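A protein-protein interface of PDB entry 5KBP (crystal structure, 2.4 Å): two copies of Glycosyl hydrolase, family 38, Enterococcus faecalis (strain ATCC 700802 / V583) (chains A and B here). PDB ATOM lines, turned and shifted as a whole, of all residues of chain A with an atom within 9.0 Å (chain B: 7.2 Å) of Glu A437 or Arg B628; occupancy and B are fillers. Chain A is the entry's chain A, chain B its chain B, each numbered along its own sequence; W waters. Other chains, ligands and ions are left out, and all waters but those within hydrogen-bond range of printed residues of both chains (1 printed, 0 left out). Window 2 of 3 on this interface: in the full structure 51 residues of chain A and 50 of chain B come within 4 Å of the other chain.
O of Ala B626 lies close to N of Glu A437 (3.3 Å).
The side-chain carboxylate (OE1) of Glu A437 is in salt-bridge range of the guanidinium group (NE) of Arg B628 (2.7 Å).
The side-chain carboxylate of Glu B622 sits at hydrogen-bond distance from the side-chain hydroxyl of Tyr A440 (3.0 Å).
The backbone NH (N) of Leu A429 lies within hydrogen-bond range of the backbone carbonyl oxygen (O) of Met A486.
The backbone carbonyl oxygen of Glu A437 lies within hydrogen-bond range of a ring nitrogen (ND1) of His A441 (3.0 Å).
The side-chain hydroxyl (OH) of Tyr A440 lies within hydrogen-bond range of the side-chain amino group (NZ) of Lys A444.
The guanidinium group of Arg B628 is in salt-bridge range of the side-chain carboxylate of Glu B623, 2.7 Å away.
NE of Arg B633 sits at hydrogen-bond distance from O of Arg B628, 3.1 Å away.
Of the printed residues of chain B, Pro A436 touches Ala B626 (3.6 Å).
Glu A437 touches just these residues of chain B: Ala B626 and Arg B628.
Printed residues of chain B within 4 Å of Tyr A440: Glu B622, Lys B625 and Ala B626.
Printed residues of chain B within 4 Å of Met A486: Lys B625 (3.6 Å), Ala B626 (3.5 Å) and Val B627 (3.6 Å).
Of the printed residues of chain A, Glu B622 touches Tyr A440 (3.0 Å).
Printed residues of chain A within 4 Å of Lys B625: Tyr A440 and Met A486.
Ala B626 touches just these residues of chain A: Pro A436 (3.6 Å), Glu A437 (3.2 Å), Tyr A440 (3.6 Å) and Met A486 (3.5 Å).
Arg B628 touches just one residue of chain A: Glu A437.
No residue of chain A comes within 4 Å of Glu B629.
The nearest residue of chain B that does not touch Glu A437 is Val B627 (4.7 Å).
The nearest residue of chain A that does not touch Arg B628 is His A441 (4.4 Å).
The nearest printed residue of chain A that does not touch Lys B625 is Val A470 (5.7 Å).
Printed residues of chain B that touch a printed residue of chain A: Glu B622, Lys B625, Ala B626, Val B627 and Arg B628.
Hydrophobic or aromatic side chains of chain B that line the printed part of chain A: Ala B626 and Val B627.
Of the 16 printed residues of chain A, 4 touch a printed residue of chain B.
Among the printed residues, 9 pairs touch across the chains.
Among the printed residues, Asp or Glu carboxylates within 4 Å of a Lys or Arg side-chain nitrogen of the other chain: Glu A437 with Arg B628.
Pro A436 touches Ala B626.
Tyr A440 touches Lys B625 (CD2 to O, 3.7 Å).
Tyr A440 touches Ala B626 (CD1 to CB, 3.6 Å).
Lys B625 touches Met A486 (O to CE, 3.6 Å).
Met A486 touches Ala B626 (CE to O, 3.5 Å).
Met A486 touches Val B627 (CE to CG2, 3.6 Å).
Water W1 lies within hydrogen-bond range of the side-chain carboxylate (OE2) of Glu A437 (2.5 Å) and the backbone NH (N) of Glu B629 (3.0 Å).
No position is printed for both chains.
Of the 9 pairs that touch across the chains among the printed residues, none has its exchanged pair printed and touching as well.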
ATOM      1  N   LEU A 429      -3.200   4.820 -25.033  1.00  0.00           N
ATOM      2  CA  LEU A 429      -2.441   4.375 -26.197  1.00  0.00           C
ATOM      3  C   LEU A 429      -3.357   4.346 -27.412  1.00  0.00           C
ATOM      4  O   LEU A 429      -4.166   3.415 -27.558  1.00  0.00           O
ATOM      5  CB  LEU A 429      -1.832   2.991 -25.954  1.00  0.00           C
ATOM      6  CG  LEU A 429      -0.910   2.815 -24.746  1.00  0.00           C
ATOM      7  CD1 LEU A 429      -0.322   1.411 -24.727  1.00  0.00           C
ATOM      8  CD2 LEU A 429       0.193   3.865 -24.739  1.00  0.00           C
ATOM      9  N   PHE A 431      -4.798   3.780 -31.237  1.00  0.00           N
ATOM     10  CA  PHE A 431      -4.653   2.591 -32.071  1.00  0.00           C
ATOM     11  C   PHE A 431      -3.556   2.751 -33.115  1.00  0.00           C
ATOM     12  O   PHE A 431      -2.932   1.757 -33.505  1.00  0.00           O
ATOM     13  CB  PHE A 431      -5.980   2.250 -32.748  1.00  0.00           C
ATOM     14  CG  PHE A 431      -6.872   1.366 -31.923  1.00  0.00           C
ATOM     15  CD1 PHE A 431      -6.637   1.188 -30.569  1.00  0.00           C
ATOM     16  CD2 PHE A 431      -7.936   0.698 -32.507  1.00  0.00           C
ATOM     17  CE1 PHE A 431      -7.456   0.371 -29.811  1.00  0.00           C
ATOM     18  CE2 PHE A 431      -8.755  -0.121 -31.755  1.00  0.00           C
ATOM     19  CZ  PHE A 431      -8.515  -0.284 -30.405  1.00  0.00           C
ATOM     20  N   GLY A 434       0.134   1.050 -32.371  1.00  0.00           N
ATOM     21  CA  GLY A 434       0.504  -0.315 -32.675  1.00  0.00           C
ATOM     22  C   GLY A 434      -0.695  -1.233 -32.724  1.00  0.00           C
ATOM     23  O   GLY A 434      -1.827  -0.797 -32.941  1.00  0.00           O
ATOM     24  N   LYS A 435      -0.426  -2.519 -32.522  1.00  0.00           N
ATOM     25  CA  LYS A 435      -1.486  -3.521 -32.547  1.00  0.00           C
ATOM     26  C   LYS A 435      -2.361  -3.377 -31.305  1.00  0.00           C
ATOM     27  O   LYS A 435      -1.832  -3.227 -30.196  1.00  0.00           O
ATOM     28  CB  LYS A 435      -0.884  -4.924 -32.624  1.00  0.00           C
ATOM     29  CG  LYS A 435      -1.905  -6.045 -32.728  1.00  0.00           C
ATOM     30  CD  LYS A 435      -1.268  -7.327 -33.243  1.00  0.00           C
ATOM     31  CE  LYS A 435      -0.775  -7.158 -34.672  1.00  0.00           C
ATOM     32  NZ  LYS A 435      -0.200  -8.416 -35.223  1.00  0.00           N
ATOM     33  N   PRO A 436      -3.690  -3.412 -31.445  1.00  0.00           N
ATOM     34  CA  PRO A 436      -4.555  -3.131 -30.285  1.00  0.00           C
ATOM     35  C   PRO A 436      -4.372  -4.092 -29.125  1.00  0.00           C
ATOM     36  O   PRO A 436      -4.414  -3.661 -27.966  1.00  0.00           O
ATOM     37  CB  PRO A 436      -5.968  -3.221 -30.881  1.00  0.00           C
ATOM     38  CG  PRO A 436      -5.784  -2.936 -32.333  1.00  0.00           C
ATOM     39  CD  PRO A 436      -4.459  -3.537 -32.694  1.00  0.00           C
ATOM     40  N   GLU A 437      -4.174  -5.386 -29.392  1.00  0.00           N
ATOM     41  CA  GLU A 437      -3.991  -6.324 -28.290  1.00  0.00           C
ATOM     42  C   GLU A 437      -2.647  -6.125 -27.604  1.00  0.00           C
ATOM     43  O   GLU A 437      -2.527  -6.369 -26.398  1.00  0.00           O
ATOM     44  CB  GLU A 437      -4.134  -7.767 -28.780  1.00  0.00           C
ATOM     45  CG  GLU A 437      -3.178  -8.169 -29.890  1.00  0.00           C
ATOM     46  CD  GLU A 437      -3.216  -9.660 -30.169  1.00  0.00           C
ATOM     47  OE1 GLU A 437      -3.373 -10.441 -29.206  1.00  0.00           O
ATOM     48  OE2 GLU A 437      -3.097 -10.053 -31.348  1.00  0.00           O
ATOM     49  N   ASP A 438      -1.629  -5.681 -28.346  1.00  0.00           N
ATOM     50  CA  ASP A 438      -0.346  -5.378 -27.722  1.00  0.00           C
ATOM     51  C   ASP A 438      -0.467  -4.191 -26.775  1.00  0.00           C
ATOM     52  O   ASP A 438       0.068  -4.222 -25.661  1.00  0.00           O
ATOM     53  CB  ASP A 438       0.714  -5.107 -28.791  1.00  0.00           C
ATOM     54  CG  ASP A 438       0.957  -6.308 -29.687  1.00  0.00           C
ATOM     55  OD1 ASP A 438       0.536  -7.423 -29.315  1.00  0.00           O
ATOM     56  OD2 ASP A 438       1.573  -6.136 -30.761  1.00  0.00           O
ATOM     57  N   LEU A 439      -1.177  -3.140 -27.197  1.00  0.00           N
ATOM     58  CA  LEU A 439      -1.391  -1.988 -26.327  1.00  0.00           C
ATOM     59  C   LEU A 439      -2.193  -2.374 -25.092  1.00  0.00           C
ATOM     60  O   LEU A 439      -1.946  -1.861 -23.994  1.00  0.00           O
ATOM     61  CB  LEU A 439      -2.105  -0.877 -27.098  1.00  0.00           C
ATOM     62  CG  LEU A 439      -1.523  -0.487 -28.458  1.00  0.00           C
ATOM     63  CD1 LEU A 439      -2.393   0.563 -29.138  1.00  0.00           C
ATOM     64  CD2 LEU A 439      -0.092   0.003 -28.312  1.00  0.00           C
ATOM     65  N   TYR A 440      -3.160  -3.278 -25.257  1.00  0.00           N
ATOM     66  CA  TYR A 440      -3.983  -3.721 -24.135  1.00  0.00           C
ATOM     67  C   TYR A 440      -3.133  -4.385 -23.060  1.00  0.00           C
ATOM     68  O   TYR A 440      -3.167  -3.988 -21.889  1.00  0.00           O
ATOM     69  CB  TYR A 440      -5.067  -4.674 -24.646  1.00  0.00           C
ATOM     70  CG  TYR A 440      -5.988  -5.239 -23.588  1.00  0.00           C
ATOM     71  CD1 TYR A 440      -5.679  -6.422 -22.930  1.00  0.00           C
ATOM     72  CD2 TYR A 440      -7.181  -4.604 -23.268  1.00  0.00           C
ATOM     73  CE1 TYR A 440      -6.521  -6.947 -21.970  1.00  0.00           C
ATOM     74  CE2 TYR A 440      -8.032  -5.122 -22.309  1.00  0.00           C
ATOM     75  CZ  TYR A 440      -7.697  -6.295 -21.664  1.00  0.00           C
ATOM     76  OH  TYR A 440      -8.537  -6.818 -20.709  1.00  0.00           O
ATOM     77  N   HIS A 441      -2.352  -5.398 -23.444  1.00  0.00           N
ATOM     78  CA  HIS A 441      -1.519  -6.100 -22.476  1.00  0.00           C
ATOM     79  C   HIS A 441      -0.318  -5.275 -22.034  1.00  0.00           C
ATOM     80  O   HIS A 441       0.223  -5.526 -20.952  1.00  0.00           O
ATOM     81  CB  HIS A 441      -1.061  -7.440 -23.054  1.00  0.00           C
ATOM     82  CG  HIS A 441      -2.176  -8.417 -23.265  1.00  0.00           C
ATOM     83  ND1 HIS A 441      -2.721  -8.671 -24.505  1.00  0.00           N
ATOM     84  CD2 HIS A 441      -2.855  -9.195 -22.389  1.00  0.00           C
ATOM     85  CE1 HIS A 441      -3.684  -9.568 -24.386  1.00  0.00           C
ATOM     86  NE2 HIS A 441      -3.785  -9.902 -23.112  1.00  0.00           N
ATOM     87  N   GLU A 442       0.110  -4.296 -22.837  1.00  0.00           N
ATOM     88  CA  GLU A 442       1.171  -3.397 -22.394  1.00  0.00           C
ATOM     89  C   GLU A 442       0.722  -2.569 -21.198  1.00  0.00           C
ATOM     90  O   GLU A 442       1.463  -2.423 -20.219  1.00  0.00           O
ATOM     91  CB  GLU A 442       1.607  -2.488 -23.543  1.00  0.00           C
ATOM     92  CG  GLU A 442       2.605  -1.415 -23.146  1.00  0.00           C
ATOM     93  CD  GLU A 442       3.020  -0.547 -24.314  1.00  0.00           C
ATOM     94  OE1 GLU A 442       3.047  -1.055 -25.455  1.00  0.00           O
ATOM     95  OE2 GLU A 442       3.313   0.647 -24.094  1.00  0.00           O
ATOM     96  N   LEU A 443      -0.494  -2.017 -21.260  1.00  0.00           N
ATOM     97  CA  LEU A 443      -1.032  -1.278 -20.123  1.00  0.00           C
ATOM     98  C   LEU A 443      -1.359  -2.202 -18.958  1.00  0.00           C
ATOM     99  O   LEU A 443      -1.223  -1.804 -17.796  1.00  0.00           O
ATOM    100  CB  LEU A 443      -2.280  -0.501 -20.544  1.00  0.00           C
ATOM    101  CG  LEU A 443      -2.089   0.587 -21.602  1.00  0.00           C
ATOM    102  CD1 LEU A 443      -3.419   1.247 -21.942  1.00  0.00           C
ATOM    103  CD2 LEU A 443      -1.082   1.621 -21.128  1.00  0.00           C
ATOM    104  N   LYS A 444      -1.791  -3.432 -19.248  1.00  0.00           N
ATOM    105  CA  LYS A 444      -2.123  -4.373 -18.183  1.00  0.00           C
ATOM    106  C   LYS A 444      -0.886  -4.751 -17.378  1.00  0.00           C
ATOM    107  O   LYS A 444      -0.965  -4.946 -16.159  1.00  0.00           O
ATOM    108  CB  LYS A 444      -2.776  -5.620 -18.779  1.00  0.00           C
ATOM    109  CG  LYS A 444      -3.646  -6.410 -17.813  1.00  0.00           C
ATOM    110  CD  LYS A 444      -5.109  -6.014 -17.946  1.00  0.00           C
ATOM    111  CE  LYS A 444      -6.015  -6.970 -17.186  1.00  0.00           C
ATOM    112  NZ  LYS A 444      -7.456  -6.667 -17.416  1.00  0.00           N
ATOM    113  N   GLN A 445       0.265  -4.851 -18.040  1.00  0.00           N
ATOM    114  CA  GLN A 445       1.510  -5.234 -17.391  1.00  0.00           C
ATOM    115  C   GLN A 445       2.273  -4.051 -16.810  1.00  0.00           C
ATOM    116  O   GLN A 445       3.209  -4.263 -16.032  1.00  0.00           O
ATOM    117  CB  GLN A 445       2.413  -5.976 -18.382  1.00  0.00           C
ATOM    118  CG  GLN A 445       1.825  -7.275 -18.906  1.00  0.00           C
ATOM    119  CD  GLN A 445       2.511  -7.752 -20.171  1.00  0.00           C
ATOM    120  OE1 GLN A 445       3.494  -7.161 -20.618  1.00  0.00           O
ATOM    121  NE2 GLN A 445       1.991  -8.823 -20.759  1.00  0.00           N
ATOM    122  N   VAL A 470      -8.011  -1.531 -17.334  1.00  0.00           N
ATOM    123  CA  VAL A 470      -7.475  -1.359 -18.678  1.00  0.00           C
ATOM    124  C   VAL A 470      -8.514  -1.889 -19.654  1.00  0.00           C
ATOM    125  O   VAL A 470      -8.821  -3.088 -19.649  1.00  0.00           O
ATOM    126  CB  VAL A 470      -6.132  -2.081 -18.862  1.00  0.00           C
ATOM    127  CG1 VAL A 470      -5.669  -1.970 -20.307  1.00  0.00           C
ATOM    128  CG2 VAL A 470      -5.087  -1.516 -17.913  1.00  0.00           C
ATOM    129  N   MET A 486      -6.568   2.218 -26.474  1.00  0.00           N
ATOM    130  CA  MET A 486      -6.556   1.445 -25.239  1.00  0.00           C
ATOM    131  C   MET A 486      -6.120   2.367 -24.109  1.00  0.00           C
ATOM    132  O   MET A 486      -5.137   3.102 -24.250  1.00  0.00           O
ATOM    133  CB  MET A 486      -5.610   0.249 -25.344  1.00  0.00           C
ATOM    134  CG  MET A 486      -6.061  -0.828 -26.311  1.00  0.00           C
ATOM    135  SD  MET A 486      -7.603  -1.609 -25.796  1.00  0.00           S
ATOM    136  CE  MET A 486      -7.614  -3.047 -26.861  1.00  0.00           C
ATOM    137  N   ILE B 568     -16.726 -18.146 -31.999  1.00  0.00           N
ATOM    138  CA  ILE B 568     -16.010 -17.139 -31.235  1.00  0.00           C
ATOM    139  C   ILE B 568     -15.751 -15.889 -32.072  1.00  0.00           C
ATOM    140  O   ILE B 568     -14.822 -15.138 -31.791  1.00  0.00           O
ATOM    141  CB  ILE B 568     -14.703 -17.705 -30.660  1.00  0.00           C
ATOM    142  CG1 ILE B 568     -13.851 -18.317 -31.775  1.00  0.00           C
ATOM    143  CG2 ILE B 568     -15.002 -18.731 -29.580  1.00  0.00           C
ATOM    144  CD1 ILE B 568     -12.523 -18.869 -31.300  1.00  0.00           C
ATOM    145  N   ARG B 619     -11.153 -17.915 -21.855  1.00  0.00           N
ATOM    146  CA  ARG B 619     -10.155 -17.193 -22.638  1.00  0.00           C
ATOM    147  C   ARG B 619     -10.775 -16.194 -23.607  1.00  0.00           C
ATOM    148  O   ARG B 619     -10.100 -15.238 -24.001  1.00  0.00           O
ATOM    149  CB  ARG B 619      -9.276 -18.178 -23.413  1.00  0.00           C
ATOM    150  CG  ARG B 619      -8.505 -19.158 -22.542  1.00  0.00           C
ATOM    151  CD  ARG B 619      -7.692 -20.129 -23.391  1.00  0.00           C
ATOM    152  NE  ARG B 619      -6.624 -19.460 -24.129  1.00  0.00           N
ATOM    153  CZ  ARG B 619      -5.353 -19.432 -23.740  1.00  0.00           C
ATOM    154  NH1 ARG B 619      -4.987 -20.043 -22.622  1.00  0.00           N
ATOM    155  NH2 ARG B 619      -4.447 -18.799 -24.472  1.00  0.00           N
ATOM    156  N   GLU B 622     -11.005 -12.078 -22.559  1.00  0.00           N
ATOM    157  CA  GLU B 622      -9.800 -11.266 -22.695  1.00  0.00           C
ATOM    158  C   GLU B 622      -9.429 -11.055 -24.156  1.00  0.00           C
ATOM    159  O   GLU B 622      -8.923  -9.989 -24.525  1.00  0.00           O
ATOM    160  CB  GLU B 622      -8.644 -11.909 -21.932  1.00  0.00           C
ATOM    161  CG  GLU B 622      -8.648 -11.595 -20.448  1.00  0.00           C
ATOM    162  CD  GLU B 622      -8.445 -10.117 -20.167  1.00  0.00           C
ATOM    163  OE1 GLU B 622      -7.366  -9.585 -20.510  1.00  0.00           O
ATOM    164  OE2 GLU B 622      -9.365  -9.485 -19.607  1.00  0.00           O
ATOM    165  N   GLU B 623      -9.670 -12.057 -25.004  1.00  0.00           N
ATOM    166  CA  GLU B 623      -9.411 -11.890 -26.429  1.00  0.00           C
ATOM    167  C   GLU B 623     -10.388 -10.905 -27.061  1.00  0.00           C
ATOM    168  O   GLU B 623     -10.044 -10.238 -28.042  1.00  0.00           O
ATOM    169  CB  GLU B 623      -9.474 -13.242 -27.141  1.00  0.00           C
ATOM    170  CG  GLU B 623      -8.495 -14.273 -26.592  1.00  0.00           C
ATOM    171  CD  GLU B 623      -8.398 -15.510 -27.462  1.00  0.00           C
ATOM    172  OE1 GLU B 623      -7.328 -15.732 -28.066  1.00  0.00           O
ATOM    173  OE2 GLU B 623      -9.394 -16.258 -27.544  1.00  0.00           O
ATOM    174  N   GLN B 624     -11.601 -10.797 -26.513  1.00  0.00           N
ATOM    175  CA  GLN B 624     -12.553  -9.802 -26.992  1.00  0.00           C
ATOM    176  C   GLN B 624     -12.187  -8.408 -26.496  1.00  0.00           C
ATOM    177  O   GLN B 624     -12.182  -7.445 -27.272  1.00  0.00           O
ATOM    178  CB  GLN B 624     -13.971 -10.167 -26.547  1.00  0.00           C
ATOM    179  CG  GLN B 624     -14.575 -11.358 -27.265  1.00  0.00           C
ATOM    180  CD  GLN B 624     -15.910 -11.772 -26.677  1.00  0.00           C
ATOM    181  OE1 GLN B 624     -16.110 -11.720 -25.462  1.00  0.00           O
ATOM    182  NE2 GLN B 624     -16.836 -12.180 -27.536  1.00  0.00           N
ATOM    183  N   LYS B 625     -11.881  -8.286 -25.202  1.00  0.00           N
ATOM    184  CA  LYS B 625     -11.544  -6.983 -24.635  1.00  0.00           C
ATOM    185  C   LYS B 625     -10.284  -6.401 -25.262  1.00  0.00           C
ATOM    186  O   LYS B 625     -10.177  -5.179 -25.416  1.00  0.00           O
ATOM    187  CB  LYS B 625     -11.373  -7.095 -23.118  1.00  0.00           C
ATOM    188  CG  LYS B 625     -12.651  -7.428 -22.365  1.00  0.00           C
ATOM    189  CD  LYS B 625     -12.440  -7.352 -20.859  1.00  0.00           C
ATOM    190  CE  LYS B 625     -13.740  -7.574 -20.103  1.00  0.00           C
ATOM    191  NZ  LYS B 625     -13.556  -7.426 -18.632  1.00  0.00           N
ATOM    192  N   ALA B 626      -9.325  -7.250 -25.627  1.00  0.00           N
ATOM    193  CA  ALA B 626      -8.077  -6.792 -26.226  1.00  0.00           C
ATOM    194  C   ALA B 626      -8.188  -6.543 -27.724  1.00  0.00           C
ATOM    195  O   ALA B 626      -7.182  -6.192 -28.350  1.00  0.00           O
ATOM    196  CB  ALA B 626      -6.961  -7.803 -25.954  1.00  0.00           C
ATOM    197  N   VAL B 627      -9.379  -6.706 -28.305  1.00  0.00           N
ATOM    198  CA  VAL B 627      -9.618  -6.510 -29.733  1.00  0.00           C
ATOM    199  C   VAL B 627      -8.645  -7.375 -30.530  1.00  0.00           C
ATOM    200  O   VAL B 627      -8.041  -6.925 -31.510  1.00  0.00           O
ATOM    201  CB  VAL B 627      -9.516  -5.022 -30.121  1.00  0.00           C
ATOM    202  CG1 VAL B 627     -10.152  -4.770 -31.483  1.00  0.00           C
ATOM    203  CG2 VAL B 627     -10.197  -4.163 -29.071  1.00  0.00           C
ATOM    204  N   ARG B 628      -8.477  -8.622 -30.101  1.00  0.00           N
ATOM    205  CA  ARG B 628      -7.670  -9.577 -30.845  1.00  0.00           C
ATOM    206  C   ARG B 628      -8.454 -10.074 -32.052  1.00  0.00           C
ATOM    207  O   ARG B 628      -9.625 -10.451 -31.927  1.00  0.00           O
ATOM    208  CB  ARG B 628      -7.266 -10.746 -29.951  1.00  0.00           C
ATOM    209  CG  ARG B 628      -6.733 -11.952 -30.708  1.00  0.00           C
ATOM    210  CD  ARG B 628      -6.243 -13.024 -29.750  1.00  0.00           C
ATOM    211  NE  ARG B 628      -5.064 -12.588 -29.009  1.00  0.00           N
ATOM    212  CZ  ARG B 628      -4.541 -13.247 -27.981  1.00  0.00           C
ATOM    213  NH1 ARG B 628      -3.463 -12.775 -27.368  1.00  0.00           N
ATOM    214  NH2 ARG B 628      -5.097 -14.374 -27.560  1.00  0.00           N
ATOM    215  N   GLU B 629      -7.813 -10.065 -33.219  1.00  0.00           N
ATOM    216  CA  GLU B 629      -8.475 -10.512 -34.437  1.00  0.00           C
ATOM    217  C   GLU B 629      -8.958 -11.950 -34.272  1.00  0.00           C
ATOM    218  O   GLU B 629      -8.283 -12.783 -33.660  1.00  0.00           O
ATOM    219  CB  GLU B 629      -7.524 -10.392 -35.629  1.00  0.00           C
ATOM    220  CG  GLU B 629      -8.216 -10.054 -36.939  1.00  0.00           C
ATOM    221  N   PHE B 630     -10.148 -12.231 -34.814  1.00  0.00           N
ATOM    222  CA  PHE B 630     -10.814 -13.498 -34.523  1.00  0.00           C
ATOM    223  C   PHE B 630     -10.033 -14.694 -35.053  1.00  0.00           C
ATOM    224  O   PHE B 630     -10.071 -15.773 -34.450  1.00  0.00           O
ATOM    225  CB  PHE B 630     -12.236 -13.494 -35.089  1.00  0.00           C
ATOM    226  CG  PHE B 630     -12.303 -13.301 -36.579  1.00  0.00           C
ATOM    227  CD1 PHE B 630     -12.373 -12.030 -37.121  1.00  0.00           C
ATOM    228  CD2 PHE B 630     -12.310 -14.392 -37.436  1.00  0.00           C
ATOM    229  CE1 PHE B 630     -12.436 -11.846 -38.489  1.00  0.00           C
ATOM    230  CE2 PHE B 630     -12.374 -14.214 -38.805  1.00  0.00           C
ATOM    231  CZ  PHE B 630     -12.438 -12.939 -39.332  1.00  0.00           C
ATOM    232  N   ARG B 631      -9.319 -14.529 -36.170  1.00  0.00           N
ATOM    233  CA  ARG B 631      -8.529 -15.627 -36.715  1.00  0.00           C
ATOM    234  C   ARG B 631      -7.385 -16.037 -35.796  1.00  0.00           C
ATOM    235  O   ARG B 631      -6.938 -17.187 -35.863  1.00  0.00           O
ATOM    236  CB  ARG B 631      -7.988 -15.247 -38.095  1.00  0.00           C
ATOM    237  CG  ARG B 631      -9.009 -15.385 -39.213  1.00  0.00           C
ATOM    238  CD  ARG B 631      -8.862 -14.283 -40.248  1.00  0.00           C
ATOM    239  NE  ARG B 631      -7.559 -14.305 -40.905  1.00  0.00           N
ATOM    240  CZ  ARG B 631      -7.146 -13.381 -41.767  1.00  0.00           C
ATOM    241  NH1 ARG B 631      -7.933 -12.360 -42.072  1.00  0.00           N
ATOM    242  NH2 ARG B 631      -5.945 -13.475 -42.319  1.00  0.00           N
ATOM    243  N   GLU B 632      -6.908 -15.134 -34.938  1.00  0.00           N
ATOM    244  CA  GLU B 632      -5.841 -15.440 -33.995  1.00  0.00           C
ATOM    245  C   GLU B 632      -6.365 -15.826 -32.617  1.00  0.00           C
ATOM    246  O   GLU B 632      -5.582 -15.895 -31.665  1.00  0.00           O
ATOM    247  CB  GLU B 632      -4.883 -14.253 -33.867  1.00  0.00           C
ATOM    248  CG  GLU B 632      -4.095 -13.935 -35.127  1.00  0.00           C
ATOM    249  CD  GLU B 632      -4.743 -12.852 -35.965  1.00  0.00           C
ATOM    250  N   ARG B 633      -7.665 -16.078 -32.485  1.00  0.00           N
ATOM    251  CA  ARG B 633      -8.238 -16.410 -31.190  1.00  0.00           C
ATOM    252  C   ARG B 633      -8.047 -17.890 -30.882  1.00  0.00           C
ATOM    253  O   ARG B 633      -8.269 -18.753 -31.735  1.00  0.00           O
ATOM    254  CB  ARG B 633      -9.720 -16.036 -31.151  1.00  0.00           C
ATOM    255  CG  ARG B 633      -9.939 -14.534 -31.096  1.00  0.00           C
ATOM    256  CD  ARG B 633     -11.405 -14.153 -31.025  1.00  0.00           C
ATOM    257  NE  ARG B 633     -11.551 -12.702 -30.969  1.00  0.00           N
ATOM    258  CZ  ARG B 633     -12.714 -12.061 -30.977  1.00  0.00           C
ATOM    259  NH1 ARG B 633     -13.853 -12.737 -31.042  1.00  0.00           N
ATOM    260  NH2 ARG B 633     -12.737 -10.736 -30.922  1.00  0.00           N
ATOM    261  N   LEU B 634      -7.621 -18.173 -29.652  1.00  0.00           N
ATOM    262  CA  LEU B 634      -7.302 -19.525 -29.216  1.00  0.00           C
ATOM    263  C   LEU B 634      -8.354 -20.114 -28.288  1.00  0.00           C
ATOM    264  O   LEU B 634      -8.176 -21.239 -27.810  1.00  0.00           O
ATOM    265  CB  LEU B 634      -5.933 -19.545 -28.521  1.00  0.00           C
ATOM    266  CG  LEU B 634      -4.672 -19.770 -29.362  1.00  0.00           C
ATOM    267  CD1 LEU B 634      -4.726 -19.049 -30.701  1.00  0.00           C
ATOM    268  CD2 LEU B 634      -3.456 -19.317 -28.577  1.00  0.00           C
ATOM    269  N   ALA B 635      -9.437 -19.389 -28.020  1.00  0.00           N
ATOM    270  CA  ALA B 635     -10.479 -19.909 -27.148  1.00  0.00           C
ATOM    271  C   ALA B 635     -11.134 -21.135 -27.769  1.00  0.00           C
ATOM    272  O   ALA B 635     -11.338 -21.204 -28.983  1.00  0.00           O
ATOM    273  CB  ALA B 635     -11.529 -18.831 -26.875  1.00  0.00           C
ATOM    274  N   GLU B 756     -20.052 -10.094 -28.955  1.00  0.00           N
ATOM    275  CA  GLU B 756     -19.477  -8.789 -29.244  1.00  0.00           C
ATOM    276  C   GLU B 756     -19.887  -8.337 -30.640  1.00  0.00           C
ATOM    277  O   GLU B 756     -20.206  -9.148 -31.514  1.00  0.00           O
ATOM    278  CB  GLU B 756     -17.947  -8.796 -29.130  1.00  0.00           C
ATOM    279  CG  GLU B 756     -17.244  -9.614 -30.200  1.00  0.00           C
ATOM    280  CD  GLU B 756     -15.779  -9.249 -30.338  1.00  0.00           C
ATOM    281  OE1 GLU B 756     -15.395  -8.157 -29.871  1.00  0.00           O
ATOM    282  OE2 GLU B 756     -15.015 -10.052 -30.911  1.00  0.00           O
HETATM  283  O   HOH W   1      -4.934  -9.439 -32.950  1.00  0.00           O
